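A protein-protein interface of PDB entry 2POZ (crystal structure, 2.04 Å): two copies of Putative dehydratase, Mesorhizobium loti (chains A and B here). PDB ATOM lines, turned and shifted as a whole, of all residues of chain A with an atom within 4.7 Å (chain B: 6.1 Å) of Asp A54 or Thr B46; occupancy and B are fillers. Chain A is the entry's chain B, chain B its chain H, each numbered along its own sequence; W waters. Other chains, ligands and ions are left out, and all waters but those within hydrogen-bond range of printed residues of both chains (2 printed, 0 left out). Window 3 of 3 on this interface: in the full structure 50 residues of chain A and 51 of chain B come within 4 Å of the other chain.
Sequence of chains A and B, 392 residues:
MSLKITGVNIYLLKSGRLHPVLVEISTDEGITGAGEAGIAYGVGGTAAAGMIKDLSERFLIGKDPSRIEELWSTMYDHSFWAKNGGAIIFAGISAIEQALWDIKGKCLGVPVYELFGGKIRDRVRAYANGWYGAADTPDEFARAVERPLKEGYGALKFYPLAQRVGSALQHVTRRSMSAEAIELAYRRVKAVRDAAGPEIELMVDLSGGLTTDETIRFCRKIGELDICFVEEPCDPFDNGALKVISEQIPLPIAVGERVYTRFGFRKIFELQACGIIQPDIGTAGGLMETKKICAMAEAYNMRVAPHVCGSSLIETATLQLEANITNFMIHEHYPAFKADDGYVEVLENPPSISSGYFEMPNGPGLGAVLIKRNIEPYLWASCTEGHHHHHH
Water W1 lies within hydrogen-bond range of N of Gly B45, N of Gly B44, NE2 of His B19 and OD2 of Asp A54.
Water W2 bridges the side-chain hydroxyl (OG1) of Thr B46 (2.7 Å) and the side-chain amino group (NZ) of Lys A53 (2.9 Å).
Of the 13 printed residues of chain B, 6 touch a printed residue of chain A.
Hydrophobic or aromatic side chains of chain B that line the printed part of chain A: Val B43, Ala B47 and Trp B380.
Among the printed residues, 13 pairs touch across the chains.
Among the printed residues, no Asp or Glu carboxylate lies within 4 Å of a Lys or Arg side-chain nitrogen of the other chain.
Trp B380 touches its own counterpart, Trp A380.
Positions printed for both chains: 50, 51 and 380.
Of the 13 pairs that touch across the chains among the printed residues, 1 has its exchanged pair printed and touching as well.
The side-chain carboxylate (OD2) of Asp A54 lies within hydrogen-bond range of the backbone NH (N) of Gly B45 (3.2 Å).
The side-chain hydroxyl (OG1) of Thr B46 lies within hydrogen-bond range of the side-chain carboxylate (OD1) of Asp A54 (2.7 Å).
The backbone carbonyl oxygen (O) of Val B43 sits close to the side-chain sulfur (SD) of Met A51 (3.8 Å).
The side-chain carboxylate of Asp A54 lies close to the backbone NH of Ala B47 (3.5 Å).
Gly A50 touches Thr B46.
C of Gly A50 touches N of Ala B47, 3.9 Å away.
Met A51 touches Gly B44 (CE to CA, 3.8 Å).
Met A51 touches Ala B47.
CG1 of Val B43 touches CB of Asp A54 (3.7 Å).
Gly B44 touches Asp A54 (C to OD2, 3.1 Å).
Leu A55 touches Val B43.
Arg A58 touches Val B43 (CG to CG2, 3.998 Å).
Trp A380 touches Trp B380 (CZ2 to CZ2, 3.97 Å).
Asp A54 touches five residues of chain B.
Printed residues of chain A within 4 Å of Thr B46: Gly A50 and Asp A54.
Of the printed residues of chain B, Arg A58 touches Val B43.
Of the printed residues of chain A, Gly B45 touches Asp A54 (3.2 Å).
Of the printed residues of chain A, Trp B380 touches Trp A380 (3.97 Å).
Of the printed residues of chain A, Val B43 touches Met A51, Asp A54, Leu A55 and Arg A58.
Of the printed residues of chain A, Gly B44 touches Met A51 and Asp A54.
The nearest residue of chain B that does not touch Asp A54 is Ala B48 (5.7 Å).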
ATOM      1  N   GLY A  50     -19.731 -19.605  -4.104  1.00  0.00           N
ATOM      2  CA  GLY A  50     -19.734 -20.644  -5.117  1.00  0.00           C
ATOM      3  C   GLY A  50     -20.979 -20.597  -5.979  1.00  0.00           C
ATOM      4  O   GLY A  50     -20.919 -20.814  -7.192  1.00  0.00           O
ATOM      5  N   MET A  51     -22.116 -20.308  -5.357  1.00  0.00           N
ATOM      6  CA  MET A  51     -23.370 -20.231  -6.088  1.00  0.00           C
ATOM      7  C   MET A  51     -23.362 -19.063  -7.073  1.00  0.00           C
ATOM      8  O   MET A  51     -23.818 -19.197  -8.208  1.00  0.00           O
ATOM      9  CB  MET A  51     -24.548 -20.066  -5.127  1.00  0.00           C
ATOM     10  CG  MET A  51     -25.892 -19.977  -5.843  1.00  0.00           C
ATOM     11  SD  MET A  51     -26.383 -21.621  -6.770  1.00  0.00           S
ATOM     12  CE  MET A  51     -25.460 -21.377  -8.430  1.00  0.00           C
ATOM     13  N   ILE A  52     -22.856 -17.914  -6.642  1.00  0.00           N
ATOM     14  CA  ILE A  52     -22.812 -16.756  -7.526  1.00  0.00           C
ATOM     15  C   ILE A  52     -21.936 -17.091  -8.732  1.00  0.00           C
ATOM     16  O   ILE A  52     -22.235 -16.700  -9.860  1.00  0.00           O
ATOM     17  CB  ILE A  52     -22.264 -15.515  -6.793  1.00  0.00           C
ATOM     18  CG1 ILE A  52     -23.203 -15.149  -5.632  1.00  0.00           C
ATOM     19  CG2 ILE A  52     -22.144 -14.350  -7.768  1.00  0.00           C
ATOM     20  CD1 ILE A  52     -22.722 -13.980  -4.781  1.00  0.00           C
ATOM     21  N   LYS A  53     -20.869 -17.845  -8.487  1.00  0.00           N
ATOM     22  CA  LYS A  53     -19.957 -18.253  -9.548  1.00  0.00           C
ATOM     23  C   LYS A  53     -20.689 -19.144 -10.551  1.00  0.00           C
ATOM     24  O   LYS A  53     -20.629 -18.912 -11.758  1.00  0.00           O
ATOM     25  CB  LYS A  53     -18.766 -19.018  -8.958  1.00  0.00           C
ATOM     26  CG  LYS A  53     -17.723 -19.468  -9.986  1.00  0.00           C
ATOM     27  CD  LYS A  53     -16.574 -20.220  -9.320  1.00  0.00           C
ATOM     28  CE  LYS A  53     -15.467 -20.575 -10.318  1.00  0.00           C
ATOM     29  NZ  LYS A  53     -15.945 -21.502 -11.386  1.00  0.00           N
ATOM     30  N   ASP A  54     -21.383 -20.159 -10.046  1.00  0.00           N
ATOM     31  CA  ASP A  54     -22.113 -21.076 -10.914  1.00  0.00           C
ATOM     32  C   ASP A  54     -23.222 -20.382 -11.706  1.00  0.00           C
ATOM     33  O   ASP A  54     -23.385 -20.634 -12.898  1.00  0.00           O
ATOM     34  CB  ASP A  54     -22.712 -22.220 -10.098  1.00  0.00           C
ATOM     35  CG  ASP A  54     -21.653 -23.152  -9.531  1.00  0.00           C
ATOM     36  OD1 ASP A  54     -20.520 -23.166 -10.066  1.00  0.00           O
ATOM     37  OD2 ASP A  54     -21.965 -23.883  -8.561  1.00  0.00           O
ATOM     38  N   LEU A  55     -23.991 -19.525 -11.040  1.00  0.00           N
ATOM     39  CA  LEU A  55     -25.067 -18.800 -11.714  1.00  0.00           C
ATOM     40  C   LEU A  55     -24.490 -17.872 -12.783  1.00  0.00           C
ATOM     41  O   LEU A  55     -25.007 -17.792 -13.902  1.00  0.00           O
ATOM     42  CB  LEU A  55     -25.866 -17.973 -10.709  1.00  0.00           C
ATOM     43  CG  LEU A  55     -26.718 -18.723  -9.684  1.00  0.00           C
ATOM     44  CD1 LEU A  55     -27.126 -17.754  -8.577  1.00  0.00           C
ATOM     45  CD2 LEU A  55     -27.943 -19.339 -10.360  1.00  0.00           C
ATOM     46  N   SER A  56     -23.414 -17.175 -12.433  1.00  0.00           N
ATOM     47  CA  SER A  56     -22.771 -16.253 -13.361  1.00  0.00           C
ATOM     48  C   SER A  56     -22.255 -16.942 -14.627  1.00  0.00           C
ATOM     49  O   SER A  56     -22.532 -16.492 -15.741  1.00  0.00           O
ATOM     50  CB  SER A  56     -21.611 -15.532 -12.667  1.00  0.00           C
ATOM     51  OG  SER A  56     -22.081 -14.673 -11.641  1.00  0.00           O
ATOM     52  N   GLU A  57     -21.516 -18.034 -14.456  1.00  0.00           N
ATOM     53  CA  GLU A  57     -20.951 -18.757 -15.595  1.00  0.00           C
ATOM     54  C   GLU A  57     -22.008 -19.384 -16.499  1.00  0.00           C
ATOM     55  O   GLU A  57     -21.807 -19.531 -17.706  1.00  0.00           O
ATOM     56  CB  GLU A  57     -19.989 -19.838 -15.099  1.00  0.00           C
ATOM     57  CG  GLU A  57     -18.866 -19.294 -14.233  1.00  0.00           C
ATOM     58  CD  GLU A  57     -17.963 -20.384 -13.691  1.00  0.00           C
ATOM     59  OE1 GLU A  57     -18.490 -21.433 -13.262  1.00  0.00           O
ATOM     60  OE2 GLU A  57     -16.731 -20.184 -13.677  1.00  0.00           O
ATOM     61  N   ARG A  58     -23.140 -19.747 -15.918  1.00  0.00           N
ATOM     62  CA  ARG A  58     -24.195 -20.366 -16.698  1.00  0.00           C
ATOM     63  C   ARG A  58     -25.204 -19.391 -17.307  1.00  0.00           C
ATOM     64  O   ARG A  58     -25.670 -19.600 -18.432  1.00  0.00           O
ATOM     65  CB  ARG A  58     -24.941 -21.387 -15.832  1.00  0.00           C
ATOM     66  CG  ARG A  58     -26.204 -21.969 -16.469  1.00  0.00           C
ATOM     67  CD  ARG A  58     -25.893 -22.809 -17.702  1.00  0.00           C
ATOM     68  NE  ARG A  58     -27.114 -23.342 -18.305  1.00  0.00           N
ATOM     69  CZ  ARG A  58     -28.002 -22.613 -18.977  1.00  0.00           C
ATOM     70  NH1 ARG A  58     -27.808 -21.311 -19.151  1.00  0.00           N
ATOM     71  NH2 ARG A  58     -29.102 -23.182 -19.460  1.00  0.00           N
ATOM     72  N   TRP A 380     -12.513 -13.722  -4.847  1.00  0.00           N
ATOM     73  CA  TRP A 380     -12.659 -15.174  -4.760  1.00  0.00           C
ATOM     74  C   TRP A 380     -12.728 -15.855  -6.124  1.00  0.00           C
ATOM     75  O   TRP A 380     -12.236 -16.971  -6.292  1.00  0.00           O
ATOM     76  CB  TRP A 380     -13.911 -15.509  -3.941  1.00  0.00           C
ATOM     77  CG  TRP A 380     -14.020 -16.934  -3.513  1.00  0.00           C
ATOM     78  CD1 TRP A 380     -13.354 -17.541  -2.483  1.00  0.00           C
ATOM     79  CD2 TRP A 380     -14.853 -17.938  -4.101  1.00  0.00           C
ATOM     80  NE1 TRP A 380     -13.726 -18.863  -2.395  1.00  0.00           N
ATOM     81  CE2 TRP A 380     -14.645 -19.131  -3.374  1.00  0.00           C
ATOM     82  CE3 TRP A 380     -15.757 -17.944  -5.169  1.00  0.00           C
ATOM     83  CZ2 TRP A 380     -15.313 -20.323  -3.683  1.00  0.00           C
ATOM     84  CZ3 TRP A 380     -16.423 -19.131  -5.478  1.00  0.00           C
ATOM     85  CH2 TRP A 380     -16.196 -20.301  -4.736  1.00  0.00           C
ATOM     86  N   LEU B  12     -14.882 -31.885  -6.318  1.00  0.00           N
ATOM     87  CA  LEU B  12     -15.860 -31.322  -7.244  1.00  0.00           C
ATOM     88  C   LEU B  12     -15.513 -31.916  -8.601  1.00  0.00           C
ATOM     89  O   LEU B  12     -14.637 -31.413  -9.306  1.00  0.00           O
ATOM     90  CB  LEU B  12     -15.747 -29.794  -7.275  1.00  0.00           C
ATOM     91  CG  LEU B  12     -16.653 -29.067  -8.277  1.00  0.00           C
ATOM     92  CD1 LEU B  12     -18.102 -29.492  -8.074  1.00  0.00           C
ATOM     93  CD2 LEU B  12     -16.506 -27.563  -8.102  1.00  0.00           C
ATOM     94  N   HIS B  19     -21.762 -33.037 -12.427  1.00  0.00           N
ATOM     95  CA  HIS B  19     -20.680 -32.460 -11.641  1.00  0.00           C
ATOM     96  C   HIS B  19     -20.833 -32.945 -10.200  1.00  0.00           C
ATOM     97  O   HIS B  19     -21.209 -32.188  -9.305  1.00  0.00           O
ATOM     98  CB  HIS B  19     -20.662 -30.921 -11.724  1.00  0.00           C
ATOM     99  CG  HIS B  19     -21.999 -30.266 -11.560  1.00  0.00           C
ATOM    100  ND1 HIS B  19     -22.724 -30.321 -10.388  1.00  0.00           N
ATOM    101  CD2 HIS B  19     -22.726 -29.503 -12.414  1.00  0.00           C
ATOM    102  CE1 HIS B  19     -23.837 -29.620 -10.527  1.00  0.00           C
ATOM    103  NE2 HIS B  19     -23.862 -29.114 -11.747  1.00  0.00           N
ATOM    104  N   VAL B  21     -20.354 -34.064  -6.406  1.00  0.00           N
ATOM    105  CA  VAL B  21     -19.681 -33.413  -5.290  1.00  0.00           C
ATOM    106  C   VAL B  21     -19.495 -34.481  -4.220  1.00  0.00           C
ATOM    107  O   VAL B  21     -20.470 -34.989  -3.665  1.00  0.00           O
ATOM    108  CB  VAL B  21     -20.538 -32.255  -4.734  1.00  0.00           C
ATOM    109  CG1 VAL B  21     -19.772 -31.498  -3.663  1.00  0.00           C
ATOM    110  CG2 VAL B  21     -20.934 -31.316  -5.874  1.00  0.00           C
ATOM    111  N   VAL B  43     -27.706 -26.132 -11.355  1.00  0.00           N
ATOM    112  CA  VAL B  43     -26.716 -25.097 -11.083  1.00  0.00           C
ATOM    113  C   VAL B  43     -26.469 -24.931  -9.585  1.00  0.00           C
ATOM    114  O   VAL B  43     -27.381 -24.596  -8.831  1.00  0.00           O
ATOM    115  CB  VAL B  43     -27.168 -23.750 -11.688  1.00  0.00           C
ATOM    116  CG1 VAL B  43     -26.132 -22.674 -11.423  1.00  0.00           C
ATOM    117  CG2 VAL B  43     -27.390 -23.913 -13.183  1.00  0.00           C
ATOM    118  N   GLY B  44     -25.225 -25.161  -9.163  1.00  0.00           N
ATOM    119  CA  GLY B  44     -24.889 -25.036  -7.755  1.00  0.00           C
ATOM    120  C   GLY B  44     -23.816 -25.989  -7.243  1.00  0.00           C
ATOM    121  O   GLY B  44     -23.544 -26.024  -6.043  1.00  0.00           O
ATOM    122  N   GLY B  45     -23.208 -26.763  -8.138  1.00  0.00           N
ATOM    123  CA  GLY B  45     -22.166 -27.687  -7.721  1.00  0.00           C
ATOM    124  C   GLY B  45     -21.074 -27.042  -6.875  1.00  0.00           C
ATOM    125  O   GLY B  45     -20.693 -27.574  -5.829  1.00  0.00           O
ATOM    126  N   THR B  46     -20.565 -25.895  -7.312  1.00  0.00           N
ATOM    127  CA  THR B  46     -19.515 -25.219  -6.560  1.00  0.00           C
ATOM    128  C   THR B  46     -20.051 -24.754  -5.204  1.00  0.00           C
ATOM    129  O   THR B  46     -19.312 -24.706  -4.216  1.00  0.00           O
ATOM    130  CB  THR B  46     -18.968 -24.008  -7.332  1.00  0.00           C
ATOM    131  OG1 THR B  46     -18.637 -24.403  -8.668  1.00  0.00           O
ATOM    132  CG2 THR B  46     -17.714 -23.479  -6.666  1.00  0.00           C
ATOM    133  N   ALA B  47     -21.337 -24.414  -5.159  1.00  0.00           N
ATOM    134  CA  ALA B  47     -21.968 -23.978  -3.915  1.00  0.00           C
ATOM    135  C   ALA B  47     -21.981 -25.137  -2.915  1.00  0.00           C
ATOM    136  O   ALA B  47     -21.695 -24.953  -1.737  1.00  0.00           O
ATOM    137  CB  ALA B  47     -23.391 -23.511  -4.189  1.00  0.00           C
ATOM    138  N   ALA B  48     -22.317 -26.331  -3.396  1.00  0.00           N
ATOM    139  CA  ALA B  48     -22.358 -27.514  -2.545  1.00  0.00           C
ATOM    140  C   ALA B  48     -20.972 -27.810  -1.980  1.00  0.00           C
ATOM    141  O   ALA B  48     -20.826 -28.125  -0.798  1.00  0.00           O
ATOM    142  CB  ALA B  48     -22.871 -28.716  -3.338  1.00  0.00           C
ATOM    143  N   ALA B  49     -19.956 -27.712  -2.832  1.00  0.00           N
ATOM    144  CA  ALA B  49     -18.582 -27.955  -2.408  1.00  0.00           C
ATOM    145  C   ALA B  49     -18.195 -26.979  -1.297  1.00  0.00           C
ATOM    146  O   ALA B  49     -17.639 -27.379  -0.271  1.00  0.00           O
ATOM    147  CB  ALA B  49     -17.638 -27.803  -3.597  1.00  0.00           C
ATOM    148  N   GLY B  50     -18.501 -25.700  -1.515  1.00  0.00           N
ATOM    149  CA  GLY B  50     -18.199 -24.666  -0.541  1.00  0.00           C
ATOM    150  C   GLY B  50     -18.953 -24.856   0.761  1.00  0.00           C
ATOM    151  O   GLY B  50     -18.447 -24.517   1.832  1.00  0.00           O
ATOM    152  N   MET B  51     -20.167 -25.392   0.686  1.00  0.00           N
ATOM    153  CA  MET B  51     -20.941 -25.617   1.897  1.00  0.00           C
ATOM    154  C   MET B  51     -20.293 -26.728   2.719  1.00  0.00           C
ATOM    155  O   MET B  51     -20.177 -26.621   3.940  1.00  0.00           O
ATOM    156  CB  MET B  51     -22.382 -26.009   1.583  1.00  0.00           C
ATOM    157  CG  MET B  51     -23.197 -26.293   2.837  1.00  0.00           C
ATOM    158  SD  MET B  51     -23.451 -24.744   4.002  1.00  0.00           S
ATOM    159  CE  MET B  51     -21.841 -24.807   5.048  1.00  0.00           C
ATOM    160  N   TRP B 380     -11.090 -30.387  -4.517  1.00  0.00           N
ATOM    161  CA  TRP B 380     -11.478 -28.976  -4.479  1.00  0.00           C
ATOM    162  C   TRP B 380     -11.029 -28.263  -3.212  1.00  0.00           C
ATOM    163  O   TRP B 380     -10.669 -27.089  -3.250  1.00  0.00           O
ATOM    164  CB  TRP B 380     -12.997 -28.857  -4.617  1.00  0.00           C
ATOM    165  CG  TRP B 380     -13.480 -27.466  -4.897  1.00  0.00           C
ATOM    166  CD1 TRP B 380     -13.453 -26.814  -6.100  1.00  0.00           C
ATOM    167  CD2 TRP B 380     -14.070 -26.556  -3.959  1.00  0.00           C
ATOM    168  NE1 TRP B 380     -13.996 -25.553  -5.969  1.00  0.00           N
ATOM    169  CE2 TRP B 380     -14.382 -25.370  -4.666  1.00  0.00           C
ATOM    170  CE3 TRP B 380     -14.368 -26.627  -2.592  1.00  0.00           C
ATOM    171  CZ2 TRP B 380     -14.977 -24.263  -4.047  1.00  0.00           C
ATOM    172  CZ3 TRP B 380     -14.961 -25.525  -1.978  1.00  0.00           C
ATOM    173  CH2 TRP B 380     -15.258 -24.359  -2.710  1.00  0.00           C
HETATM  174  O   HOH W   1     -23.022 -26.165 -10.739  1.00  0.00           O
HETATM  175  O   HOH W   2     -16.322 -24.003  -9.985  1.00  0.00           O
